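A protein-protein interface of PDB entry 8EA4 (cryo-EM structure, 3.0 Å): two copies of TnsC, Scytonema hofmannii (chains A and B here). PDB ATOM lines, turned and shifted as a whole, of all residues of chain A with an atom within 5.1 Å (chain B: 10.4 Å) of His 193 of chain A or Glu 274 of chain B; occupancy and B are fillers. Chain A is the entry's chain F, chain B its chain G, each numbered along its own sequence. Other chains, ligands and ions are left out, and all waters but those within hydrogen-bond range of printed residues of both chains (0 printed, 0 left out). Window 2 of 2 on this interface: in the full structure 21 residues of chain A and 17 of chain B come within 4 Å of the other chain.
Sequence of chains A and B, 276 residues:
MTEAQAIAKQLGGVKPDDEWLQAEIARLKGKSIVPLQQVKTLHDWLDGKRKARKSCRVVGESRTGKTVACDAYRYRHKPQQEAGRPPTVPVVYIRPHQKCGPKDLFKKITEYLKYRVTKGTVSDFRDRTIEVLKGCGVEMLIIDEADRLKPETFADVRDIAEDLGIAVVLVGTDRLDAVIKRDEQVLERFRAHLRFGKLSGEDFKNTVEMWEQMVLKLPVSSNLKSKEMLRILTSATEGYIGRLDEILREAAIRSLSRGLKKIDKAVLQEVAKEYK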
ATOM      1  N   TRP A  45      -0.005   1.466  22.938  1.00  0.00           N
ATOM      2  CA  TRP A  45      -0.131   2.900  23.162  1.00  0.00           C
ATOM      3  C   TRP A  45       0.671   3.357  24.380  1.00  0.00           C
ATOM      4  O   TRP A  45       1.495   4.258  24.258  1.00  0.00           O
ATOM      5  CB  TRP A  45      -1.612   3.248  23.264  1.00  0.00           C
ATOM      6  CG  TRP A  45      -1.927   4.696  23.421  1.00  0.00           C
ATOM      7  CD1 TRP A  45      -1.920   5.604  22.426  1.00  0.00           C
ATOM      8  CD2 TRP A  45      -2.295   5.428  24.623  1.00  0.00           C
ATOM      9  NE1 TRP A  45      -2.279   6.837  22.926  1.00  0.00           N
ATOM     10  CE2 TRP A  45      -2.578   6.774  24.262  1.00  0.00           C
ATOM     11  CE3 TRP A  45      -2.423   5.098  25.982  1.00  0.00           C
ATOM     12  CZ2 TRP A  45      -3.045   7.720  25.181  1.00  0.00           C
ATOM     13  CZ3 TRP A  45      -2.847   6.050  26.922  1.00  0.00           C
ATOM     14  CH2 TRP A  45      -3.200   7.342  26.519  1.00  0.00           C
ATOM     15  N   LYS A  49       4.011   6.046  25.055  1.00  0.00           N
ATOM     16  CA  LYS A  49       4.014   7.093  26.092  1.00  0.00           C
ATOM     17  C   LYS A  49       5.119   6.908  27.132  1.00  0.00           C
ATOM     18  O   LYS A  49       5.694   7.889  27.585  1.00  0.00           O
ATOM     19  CB  LYS A  49       2.641   7.169  26.775  1.00  0.00           C
ATOM     20  CG  LYS A  49       1.480   7.449  25.816  1.00  0.00           C
ATOM     21  CD  LYS A  49       1.526   8.831  25.179  1.00  0.00           C
ATOM     22  CE  LYS A  49       0.393   8.934  24.170  1.00  0.00           C
ATOM     23  NZ  LYS A  49       0.450  10.191  23.394  1.00  0.00           N
ATOM     24  N   CYS A  56      -0.770  11.570  29.620  1.00  0.00           N
ATOM     25  CA  CYS A  56      -1.963  11.288  28.842  1.00  0.00           C
ATOM     26  C   CYS A  56      -3.069  10.734  29.739  1.00  0.00           C
ATOM     27  O   CYS A  56      -2.877  10.571  30.941  1.00  0.00           O
ATOM     28  CB  CYS A  56      -1.584  10.310  27.729  1.00  0.00           C
ATOM     29  SG  CYS A  56      -0.896   8.801  28.429  1.00  0.00           S
ATOM     30  N   ARG A  57      -4.244  10.444  29.193  1.00  0.00           N
ATOM     31  CA  ARG A  57      -5.295   9.774  29.956  1.00  0.00           C
ATOM     32  C   ARG A  57      -5.993   8.669  29.187  1.00  0.00           C
ATOM     33  O   ARG A  57      -6.106   8.722  27.976  1.00  0.00           O
ATOM     34  CB  ARG A  57      -6.231  10.815  30.561  1.00  0.00           C
ATOM     35  CG  ARG A  57      -7.076  11.539  29.532  1.00  0.00           C
ATOM     36  CD  ARG A  57      -7.877  12.640  30.212  1.00  0.00           C
ATOM     37  NE  ARG A  57      -9.030  13.037  29.399  1.00  0.00           N
ATOM     38  CZ  ARG A  57      -9.051  13.567  28.205  1.00  0.00           C
ATOM     39  NH1 ARG A  57      -7.975  13.968  27.619  1.00  0.00           N
ATOM     40  NH2 ARG A  57     -10.176  13.710  27.586  1.00  0.00           N
ATOM     41  N   VAL A  59      -9.639   6.863  28.975  1.00  0.00           N
ATOM     42  CA  VAL A  59     -11.022   7.111  29.345  1.00  0.00           C
ATOM     43  C   VAL A  59     -11.877   6.018  28.772  1.00  0.00           C
ATOM     44  O   VAL A  59     -11.491   5.364  27.825  1.00  0.00           O
ATOM     45  CB  VAL A  59     -11.525   8.433  28.782  1.00  0.00           C
ATOM     46  CG1 VAL A  59     -10.716   9.574  29.345  1.00  0.00           C
ATOM     47  CG2 VAL A  59     -11.425   8.419  27.279  1.00  0.00           C
ATOM     48  N   ARG A 191      -4.342  16.210  27.795  1.00  0.00           N
ATOM     49  CA  ARG A 191      -5.272  16.183  26.658  1.00  0.00           C
ATOM     50  C   ARG A 191      -5.159  14.916  25.816  1.00  0.00           C
ATOM     51  O   ARG A 191      -6.177  14.388  25.387  1.00  0.00           O
ATOM     52  CB  ARG A 191      -5.116  17.450  25.815  1.00  0.00           C
ATOM     53  CG  ARG A 191      -6.025  17.367  24.585  1.00  0.00           C
ATOM     54  CD  ARG A 191      -6.351  18.735  24.014  1.00  0.00           C
ATOM     55  NE  ARG A 191      -7.555  19.321  24.642  1.00  0.00           N
ATOM     56  CZ  ARG A 191      -8.805  19.061  24.298  1.00  0.00           C
ATOM     57  NH1 ARG A 191      -9.121  18.212  23.372  1.00  0.00           N
ATOM     58  NH2 ARG A 191      -9.787  19.661  24.885  1.00  0.00           N
ATOM     59  N   ALA A 192      -3.952  14.427  25.572  1.00  0.00           N
ATOM     60  CA  ALA A 192      -3.743  13.231  24.767  1.00  0.00           C
ATOM     61  C   ALA A 192      -4.480  12.045  25.380  1.00  0.00           C
ATOM     62  O   ALA A 192      -4.309  11.792  26.567  1.00  0.00           O
ATOM     63  CB  ALA A 192      -2.247  12.960  24.703  1.00  0.00           C
ATOM     64  N   HIS A 193      -5.275  11.301  24.620  1.00  0.00           N
ATOM     65  CA  HIS A 193      -6.026  10.188  25.194  1.00  0.00           C
ATOM     66  C   HIS A 193      -6.241   9.006  24.263  1.00  0.00           C
ATOM     67  O   HIS A 193      -6.352   9.137  23.049  1.00  0.00           O
ATOM     68  CB  HIS A 193      -7.372  10.672  25.736  1.00  0.00           C
ATOM     69  CG  HIS A 193      -8.350  11.078  24.674  1.00  0.00           C
ATOM     70  ND1 HIS A 193      -8.347  12.244  23.970  1.00  0.00           N
ATOM     71  CD2 HIS A 193      -9.353  10.314  24.166  1.00  0.00           C
ATOM     72  CE1 HIS A 193      -9.333  12.195  23.068  1.00  0.00           C
ATOM     73  NE2 HIS A 193      -9.981  11.031  23.149  1.00  0.00           N
ATOM     74  N   LEU A 194      -6.388   7.844  24.884  1.00  0.00           N
ATOM     75  CA  LEU A 194      -6.954   6.652  24.280  1.00  0.00           C
ATOM     76  C   LEU A 194      -8.312   6.385  24.911  1.00  0.00           C
ATOM     77  O   LEU A 194      -8.445   6.430  26.127  1.00  0.00           O
ATOM     78  CB  LEU A 194      -5.962   5.502  24.442  1.00  0.00           C
ATOM     79  CG  LEU A 194      -6.499   4.156  23.949  1.00  0.00           C
ATOM     80  CD1 LEU A 194      -5.397   3.323  23.332  1.00  0.00           C
ATOM     81  CD2 LEU A 194      -7.066   3.339  25.092  1.00  0.00           C
ATOM     82  N   ARG A 195      -9.321   6.094  24.094  1.00  0.00           N
ATOM     83  CA  ARG A 195     -10.643   5.680  24.551  1.00  0.00           C
ATOM     84  C   ARG A 195     -11.015   4.225  24.346  1.00  0.00           C
ATOM     85  O   ARG A 195     -10.905   3.704  23.255  1.00  0.00           O
ATOM     86  CB  ARG A 195     -11.697   6.533  23.860  1.00  0.00           C
ATOM     87  CG  ARG A 195     -13.133   6.221  24.257  1.00  0.00           C
ATOM     88  CD  ARG A 195     -14.095   7.141  23.601  1.00  0.00           C
ATOM     89  NE  ARG A 195     -13.916   8.515  24.041  1.00  0.00           N
ATOM     90  CZ  ARG A 195     -14.449   9.036  25.165  1.00  0.00           C
ATOM     91  NH1 ARG A 195     -15.189   8.282  25.948  1.00  0.00           N
ATOM     92  NH2 ARG A 195     -14.226  10.299  25.478  1.00  0.00           N
ATOM     93  N   ILE B 232      -3.074  20.392   9.150  1.00  0.00           N
ATOM     94  CA  ILE B 232      -3.050  19.359  10.139  1.00  0.00           C
ATOM     95  C   ILE B 232      -2.599  19.913  11.450  1.00  0.00           C
ATOM     96  O   ILE B 232      -3.191  19.604  12.431  1.00  0.00           O
ATOM     97  CB  ILE B 232      -2.128  18.202   9.718  1.00  0.00           C
ATOM     98  CG1 ILE B 232      -2.673  17.510   8.465  1.00  0.00           C
ATOM     99  CG2 ILE B 232      -1.974  17.202  10.855  1.00  0.00           C
ATOM    100  CD1 ILE B 232      -1.683  16.584   7.798  1.00  0.00           C
ATOM    101  N   SER B 235      -5.109  22.577  13.256  1.00  0.00           N
ATOM    102  CA  SER B 235      -6.185  21.949  13.983  1.00  0.00           C
ATOM    103  C   SER B 235      -5.650  21.228  15.204  1.00  0.00           C
ATOM    104  O   SER B 235      -6.231  21.304  16.278  1.00  0.00           O
ATOM    105  CB  SER B 235      -6.926  20.974  13.087  1.00  0.00           C
ATOM    106  OG  SER B 235      -7.969  20.346  13.784  1.00  0.00           O
ATOM    107  N   ALA B 236      -4.541  20.526  15.047  1.00  0.00           N
ATOM    108  CA  ALA B 236      -3.935  19.833  16.170  1.00  0.00           C
ATOM    109  C   ALA B 236      -3.433  20.696  17.315  1.00  0.00           C
ATOM    110  O   ALA B 236      -3.548  20.293  18.464  1.00  0.00           O
ATOM    111  CB  ALA B 236      -2.824  18.919  15.687  1.00  0.00           C
ATOM    112  N   THR B 237      -2.872  21.865  17.018  1.00  0.00           N
ATOM    113  CA  THR B 237      -2.208  22.673  18.045  1.00  0.00           C
ATOM    114  C   THR B 237      -2.905  23.919  18.567  1.00  0.00           C
ATOM    115  O   THR B 237      -2.574  24.395  19.639  1.00  0.00           O
ATOM    116  CB  THR B 237      -0.825  23.107  17.530  1.00  0.00           C
ATOM    117  OG1 THR B 237      -0.981  23.972  16.397  1.00  0.00           O
ATOM    118  CG2 THR B 237      -0.003  21.893  17.123  1.00  0.00           C
ATOM    119  N   ARG B 243       1.745  22.545  22.469  1.00  0.00           N
ATOM    120  CA  ARG B 243       1.320  21.464  21.654  1.00  0.00           C
ATOM    121  C   ARG B 243       2.154  21.344  20.448  1.00  0.00           C
ATOM    122  O   ARG B 243       2.526  20.271  20.105  1.00  0.00           O
ATOM    123  CB  ARG B 243      -0.133  21.638  21.240  1.00  0.00           C
ATOM    124  CG  ARG B 243      -1.143  21.462  22.360  1.00  0.00           C
ATOM    125  CD  ARG B 243      -2.532  21.704  21.892  1.00  0.00           C
ATOM    126  NE  ARG B 243      -3.505  21.511  22.954  1.00  0.00           N
ATOM    127  CZ  ARG B 243      -4.804  21.867  22.879  1.00  0.00           C
ATOM    128  NH1 ARG B 243      -5.267  22.429  21.786  1.00  0.00           N
ATOM    129  NH2 ARG B 243      -5.607  21.648  23.904  1.00  0.00           N
ATOM    130  N   GLU B 246       5.263  19.361  21.349  1.00  0.00           N
ATOM    131  CA  GLU B 246       4.932  18.003  21.730  1.00  0.00           C
ATOM    132  C   GLU B 246       4.538  17.147  20.520  1.00  0.00           C
ATOM    133  O   GLU B 246       5.021  16.028  20.377  1.00  0.00           O
ATOM    134  CB  GLU B 246       3.833  18.146  22.780  1.00  0.00           C
ATOM    135  CG  GLU B 246       3.408  16.837  23.418  1.00  0.00           C
ATOM    136  CD  GLU B 246       2.362  17.081  24.512  1.00  0.00           C
ATOM    137  OE1 GLU B 246       2.527  17.999  25.338  1.00  0.00           O
ATOM    138  OE2 GLU B 246       1.364  16.342  24.549  1.00  0.00           O
ATOM    139  N   ILE B 247       3.736  17.689  19.597  1.00  0.00           N
ATOM    140  CA  ILE B 247       3.336  17.000  18.416  1.00  0.00           C
ATOM    141  C   ILE B 247       4.420  16.788  17.432  1.00  0.00           C
ATOM    142  O   ILE B 247       4.500  15.717  16.991  1.00  0.00           O
ATOM    143  CB  ILE B 247       2.193  17.760  17.721  1.00  0.00           C
ATOM    144  CG1 ILE B 247       0.947  17.780  18.615  1.00  0.00           C
ATOM    145  CG2 ILE B 247       1.872  17.129  16.375  1.00  0.00           C
ATOM    146  CD1 ILE B 247       0.364  16.411  18.883  1.00  0.00           C
ATOM    147  N   GLU B 250       6.812  13.941  18.978  1.00  0.00           N
ATOM    148  CA  GLU B 250       6.206  12.615  18.826  1.00  0.00           C
ATOM    149  C   GLU B 250       6.222  12.160  17.360  1.00  0.00           C
ATOM    150  O   GLU B 250       6.666  11.050  17.075  1.00  0.00           O
ATOM    151  CB  GLU B 250       4.786  12.643  19.402  1.00  0.00           C
ATOM    152  CG  GLU B 250       3.994  11.338  19.243  1.00  0.00           C
ATOM    153  CD  GLU B 250       4.576  10.137  19.998  1.00  0.00           C
ATOM    154  OE1 GLU B 250       5.207  10.330  21.052  1.00  0.00           O
ATOM    155  OE2 GLU B 250       4.322   8.995  19.564  1.00  0.00           O
ATOM    156  N   ALA B 251       5.827  13.010  16.403  1.00  0.00           N
ATOM    157  CA  ALA B 251       5.878  12.649  15.000  1.00  0.00           C
ATOM    158  C   ALA B 251       7.244  12.354  14.424  1.00  0.00           C
ATOM    159  O   ALA B 251       7.369  11.365  13.795  1.00  0.00           O
ATOM    160  CB  ALA B 251       5.173  13.653  14.130  1.00  0.00           C
ATOM    161  N   ARG B 254       8.297   8.793  16.232  1.00  0.00           N
ATOM    162  CA  ARG B 254       7.523   7.685  15.679  1.00  0.00           C
ATOM    163  C   ARG B 254       8.029   7.325  14.289  1.00  0.00           C
ATOM    164  O   ARG B 254       8.215   6.151  13.983  1.00  0.00           O
ATOM    165  CB  ARG B 254       6.041   8.091  15.707  1.00  0.00           C
ATOM    166  CG  ARG B 254       5.116   6.901  15.445  1.00  0.00           C
ATOM    167  CD  ARG B 254       3.638   7.265  15.585  1.00  0.00           C
ATOM    168  NE  ARG B 254       3.268   7.622  16.966  1.00  0.00           N
ATOM    169  CZ  ARG B 254       2.059   7.579  17.488  1.00  0.00           C
ATOM    170  NH1 ARG B 254       1.029   7.061  16.891  1.00  0.00           N
ATOM    171  NH2 ARG B 254       1.867   8.074  18.661  1.00  0.00           N
ATOM    172  N   ARG B 258      10.497   3.831  12.227  1.00  0.00           N
ATOM    173  CA  ARG B 258       9.979   3.102  11.066  1.00  0.00           C
ATOM    174  C   ARG B 258      10.822   3.314   9.820  1.00  0.00           C
ATOM    175  O   ARG B 258      10.425   2.920   8.729  1.00  0.00           O
ATOM    176  CB  ARG B 258       8.550   3.529  10.772  1.00  0.00           C
ATOM    177  CG  ARG B 258       7.541   3.173  11.852  1.00  0.00           C
ATOM    178  CD  ARG B 258       6.180   3.670  11.513  1.00  0.00           C
ATOM    179  NE  ARG B 258       5.228   3.415  12.586  1.00  0.00           N
ATOM    180  CZ  ARG B 258       3.997   3.949  12.657  1.00  0.00           C
ATOM    181  NH1 ARG B 258       3.577   4.764  11.718  1.00  0.00           N
ATOM    182  NH2 ARG B 258       3.207   3.653  13.675  1.00  0.00           N
ATOM    183  N   ALA B 266       0.163  11.143   6.473  1.00  0.00           N
ATOM    184  CA  ALA B 266      -0.513  10.167   7.302  1.00  0.00           C
ATOM    185  C   ALA B 266       0.102  10.007   8.689  1.00  0.00           C
ATOM    186  O   ALA B 266      -0.626   9.857   9.644  1.00  0.00           O
ATOM    187  CB  ALA B 266      -0.578   8.833   6.605  1.00  0.00           C
ATOM    188  N   VAL B 267       1.421  10.053   8.823  1.00  0.00           N
ATOM    189  CA  VAL B 267       2.033   9.727  10.143  1.00  0.00           C
ATOM    190  C   VAL B 267       1.715  10.862  11.120  1.00  0.00           C
ATOM    191  O   VAL B 267       1.547  10.580  12.321  1.00  0.00           O
ATOM    192  CB  VAL B 267       3.561   9.557  10.029  1.00  0.00           C
ATOM    193  CG1 VAL B 267       4.171   9.324  11.404  1.00  0.00           C
ATOM    194  CG2 VAL B 267       3.885   8.405   9.092  1.00  0.00           C
ATOM    195  N   LEU B 268       1.624  12.106  10.654  1.00  0.00           N
ATOM    196  CA  LEU B 268       1.356  13.242  11.507  1.00  0.00           C
ATOM    197  C   LEU B 268      -0.115  13.247  11.881  1.00  0.00           C
ATOM    198  O   LEU B 268      -0.454  13.579  13.007  1.00  0.00           O
ATOM    199  CB  LEU B 268       1.798  14.515  10.777  1.00  0.00           C
ATOM    200  CG  LEU B 268       1.659  15.807  11.582  1.00  0.00           C
ATOM    201  CD1 LEU B 268       2.416  15.776  12.881  1.00  0.00           C
ATOM    202  CD2 LEU B 268       2.193  16.958  10.755  1.00  0.00           C
ATOM    203  N   GLN B 269      -0.988  12.795  10.987  1.00  0.00           N
ATOM    204  CA  GLN B 269      -2.434  12.644  11.311  1.00  0.00           C
ATOM    205  C   GLN B 269      -2.605  11.519  12.339  1.00  0.00           C
ATOM    206  O   GLN B 269      -3.468  11.661  13.228  1.00  0.00           O
ATOM    207  CB  GLN B 269      -3.260  12.337  10.055  1.00  0.00           C
ATOM    208  CG  GLN B 269      -3.423  13.519   9.117  1.00  0.00           C
ATOM    209  CD  GLN B 269      -4.267  13.183   7.906  1.00  0.00           C
ATOM    210  OE1 GLN B 269      -3.865  12.386   7.053  1.00  0.00           O
ATOM    211  NE2 GLN B 269      -5.446  13.789   7.817  1.00  0.00           N
ATOM    212  N   GLU B 270      -1.827  10.444  12.186  1.00  0.00           N
ATOM    213  CA  GLU B 270      -1.821   9.315  13.153  1.00  0.00           C
ATOM    214  C   GLU B 270      -1.550   9.865  14.558  1.00  0.00           C
ATOM    215  O   GLU B 270      -2.296   9.499  15.487  1.00  0.00           O
ATOM    216  CB  GLU B 270      -0.762   8.272  12.781  1.00  0.00           C
ATOM    217  CG  GLU B 270      -0.652   7.112  13.759  1.00  0.00           C
ATOM    218  CD  GLU B 270       0.452   6.155  13.411  1.00  0.00           C
ATOM    219  OE1 GLU B 270       0.739   6.009  12.249  1.00  0.00           O
ATOM    220  OE2 GLU B 270       1.006   5.567  14.310  1.00  0.00           O
ATOM    221  N   VAL B 271      -0.559  10.747  14.700  1.00  0.00           N
ATOM    222  CA  VAL B 271      -0.235  11.361  16.024  1.00  0.00           C
ATOM    223  C   VAL B 271      -1.346  12.351  16.419  1.00  0.00           C
ATOM    224  O   VAL B 271      -1.861  12.241  17.545  1.00  0.00           O
ATOM    225  CB  VAL B 271       1.116  12.101  15.975  1.00  0.00           C
ATOM    226  CG1 VAL B 271       1.346  12.871  17.265  1.00  0.00           C
ATOM    227  CG2 VAL B 271       2.241  11.108  15.733  1.00  0.00           C
ATOM    228  N   ALA B 272      -1.717  13.259  15.511  1.00  0.00           N
ATOM    229  CA  ALA B 272      -2.670  14.334  15.859  1.00  0.00           C
ATOM    230  C   ALA B 272      -3.986  13.722  16.358  1.00  0.00           C
ATOM    231  O   ALA B 272      -4.588  14.288  17.295  1.00  0.00           O
ATOM    232  CB  ALA B 272      -2.895  15.232  14.666  1.00  0.00           C
ATOM    233  N   LYS B 273      -4.412  12.611  15.749  1.00  0.00           N
ATOM    234  CA  LYS B 273      -5.703  11.953  16.101  1.00  0.00           C
ATOM    235  C   LYS B 273      -5.728  11.562  17.582  1.00  0.00           C
ATOM    236  O   LYS B 273      -6.840  11.426  18.134  1.00  0.00           O
ATOM    237  CB  LYS B 273      -5.941  10.716  15.229  1.00  0.00           C
ATOM    238  CG  LYS B 273      -7.307  10.068  15.418  1.00  0.00           C
ATOM    239  CD  LYS B 273      -7.515   8.922  14.437  1.00  0.00           C
ATOM    240  CE  LYS B 273      -8.864   8.253  14.648  1.00  0.00           C
ATOM    241  NZ  LYS B 273      -9.074   7.122  13.704  1.00  0.00           N
ATOM    242  N   GLU B 274      -4.629  11.532  18.336  1.00  0.00           N
ATOM    243  CA  GLU B 274      -4.644  11.347  19.810  1.00  0.00           C
ATOM    244  C   GLU B 274      -5.073  12.571  20.659  1.00  0.00           C
ATOM    245  O   GLU B 274      -5.246  12.436  21.864  1.00  0.00           O
ATOM    246  CB  GLU B 274      -3.264  10.864  20.292  1.00  0.00           C
ATOM    247  CG  GLU B 274      -2.820   9.544  19.647  1.00  0.00           C
ATOM    248  CD  GLU B 274      -1.451   9.069  20.133  1.00  0.00           C
ATOM    249  OE1 GLU B 274      -1.048   9.428  21.249  1.00  0.00           O
ATOM    250  OE2 GLU B 274      -0.784   8.292  19.416  1.00  0.00           O
ATOM    251  N   TYR B 275      -5.230  13.767  20.087  1.00  0.00           N
ATOM    252  CA  TYR B 275      -5.441  15.021  20.840  1.00  0.00           C
ATOM    253  C   TYR B 275      -6.854  15.566  20.646  1.00  0.00           C
ATOM    254  O   TYR B 275      -7.291  16.420  21.414  1.00  0.00           O
ATOM    255  CB  TYR B 275      -4.386  16.072  20.457  1.00  0.00           C
ATOM    256  CG  TYR B 275      -2.999  15.772  20.987  1.00  0.00           C
ATOM    257  CD1 TYR B 275      -2.270  14.676  20.485  1.00  0.00           C
ATOM    258  CD2 TYR B 275      -2.448  16.570  22.001  1.00  0.00           C
ATOM    259  CE1 TYR B 275      -1.036  14.324  21.046  1.00  0.00           C
ATOM    260  CE2 TYR B 275      -1.202  16.234  22.552  1.00  0.00           C
ATOM    261  CZ  TYR B 275      -0.501  15.101  22.083  1.00  0.00           C
ATOM    262  OH  TYR B 275       0.687  14.748  22.627  1.00  0.00           O
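OE1 of Glu 274 of chain B lies within hydrogen-bond range of NE1 of Trp 45 of chain A (3.3 Å). The side-chain amino group (NZ) of Lys 49 of chain A is in salt-bridge range of the side-chain carboxylate (OE1) of Glu 274 of chain B, 2.7 Å away. O of Tyr 275 of chain B sits at hydrogen-bond distance from NH1 of Arg 191 of chain A. N of His 193 of chain A is in hydrogen-bond range of O of Glu 274 of chain B. The guanidinium group (NH2) of Arg 243 of chain B sits close to the guanidinium group (NE) of Arg 191 of chain A, 3.1 Å away.
NH1 of Arg 57 of chain A sits at hydrogen-bond distance from O of Arg 191 of chain A (2.9 Å). N of Arg 57 of chain A lies within hydrogen-bond range of O of Ala 192 of chain A (3.0 Å). O of Arg 191 of chain A lies within hydrogen-bond range of ND1 of His 193 of chain A (3.4 Å). The side-chain carboxylate of Glu 246 of chain B sits at hydrogen-bond distance from the side-chain hydroxyl of Tyr 275 of chain B (2.6 Å). The side-chain carboxylate of Glu 274 of chain B lies within salt-bridge range of the guanidinium group of Arg 254 of chain B, 2.8 Å away.
Glu 274 of chain B touches Ala 192 of chain A (O to CA, 3.4 Å). Tyr 275 of chain B touches Ala 192 of chain A (CZ to CB, 3.8 Å).
Of chain B, only Glu 274 comes within 4 Å of His 193 of chain A. Of the printed residues of chain A, Glu 274 of chain B touches Trp 45 (3.3 Å), Lys 49 (2.7 Å), Ala 192 (3.4 Å) and His 193 (3.0 Å). No residue of chain B comes within 4 Å of Arg 57 of chain A. Ala 192 of chain A touches just these residues of chain B: Glu 274 and Tyr 275. No residue of chain B comes within 4 Å of Leu 194 of chain A. Of the printed residues of chain B, Arg 191 of chain A touches Arg 243 and Tyr 275. Printed residues of chain A within 4 Å of Tyr 275 of chain B: Arg 191 and Ala 192. Printed residues of chain A within 4 Å of Arg 243 of chain B: Arg 191. Printed residues of chain B within 4 Å of Lys 49 of chain A: Glu 274. Val 271 of chain B touches none of the printed residues of chain A. The nearest residue of chain B that does not touch His 193 of chain A is Tyr 275 of chain B (4.8 Å). The nearest printed residue of chain B that does not touch Lys 49 of chain A is Tyr 275 of chain B (4.6 Å).
Hydrophobic or aromatic side chains of chain A within 4 Å of the printed part of chain B: Trp 45, Ala 192 and His 193. Of the 21 printed residues of chain B, 3 touch a printed residue of chain A. Printed residues of chain B that touch a printed residue of chain A: Arg 243, Glu 274 and Tyr 275. Hydrophobic or aromatic side chains of chain B that line the printed part of chain A: Tyr 275. Among the printed residues, 7 pairs touch across the chains.
No position is printed for both chains. Of the 7 pairs that touch across the chains among the printed residues, none has its exchanged pair printed and touching as well.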
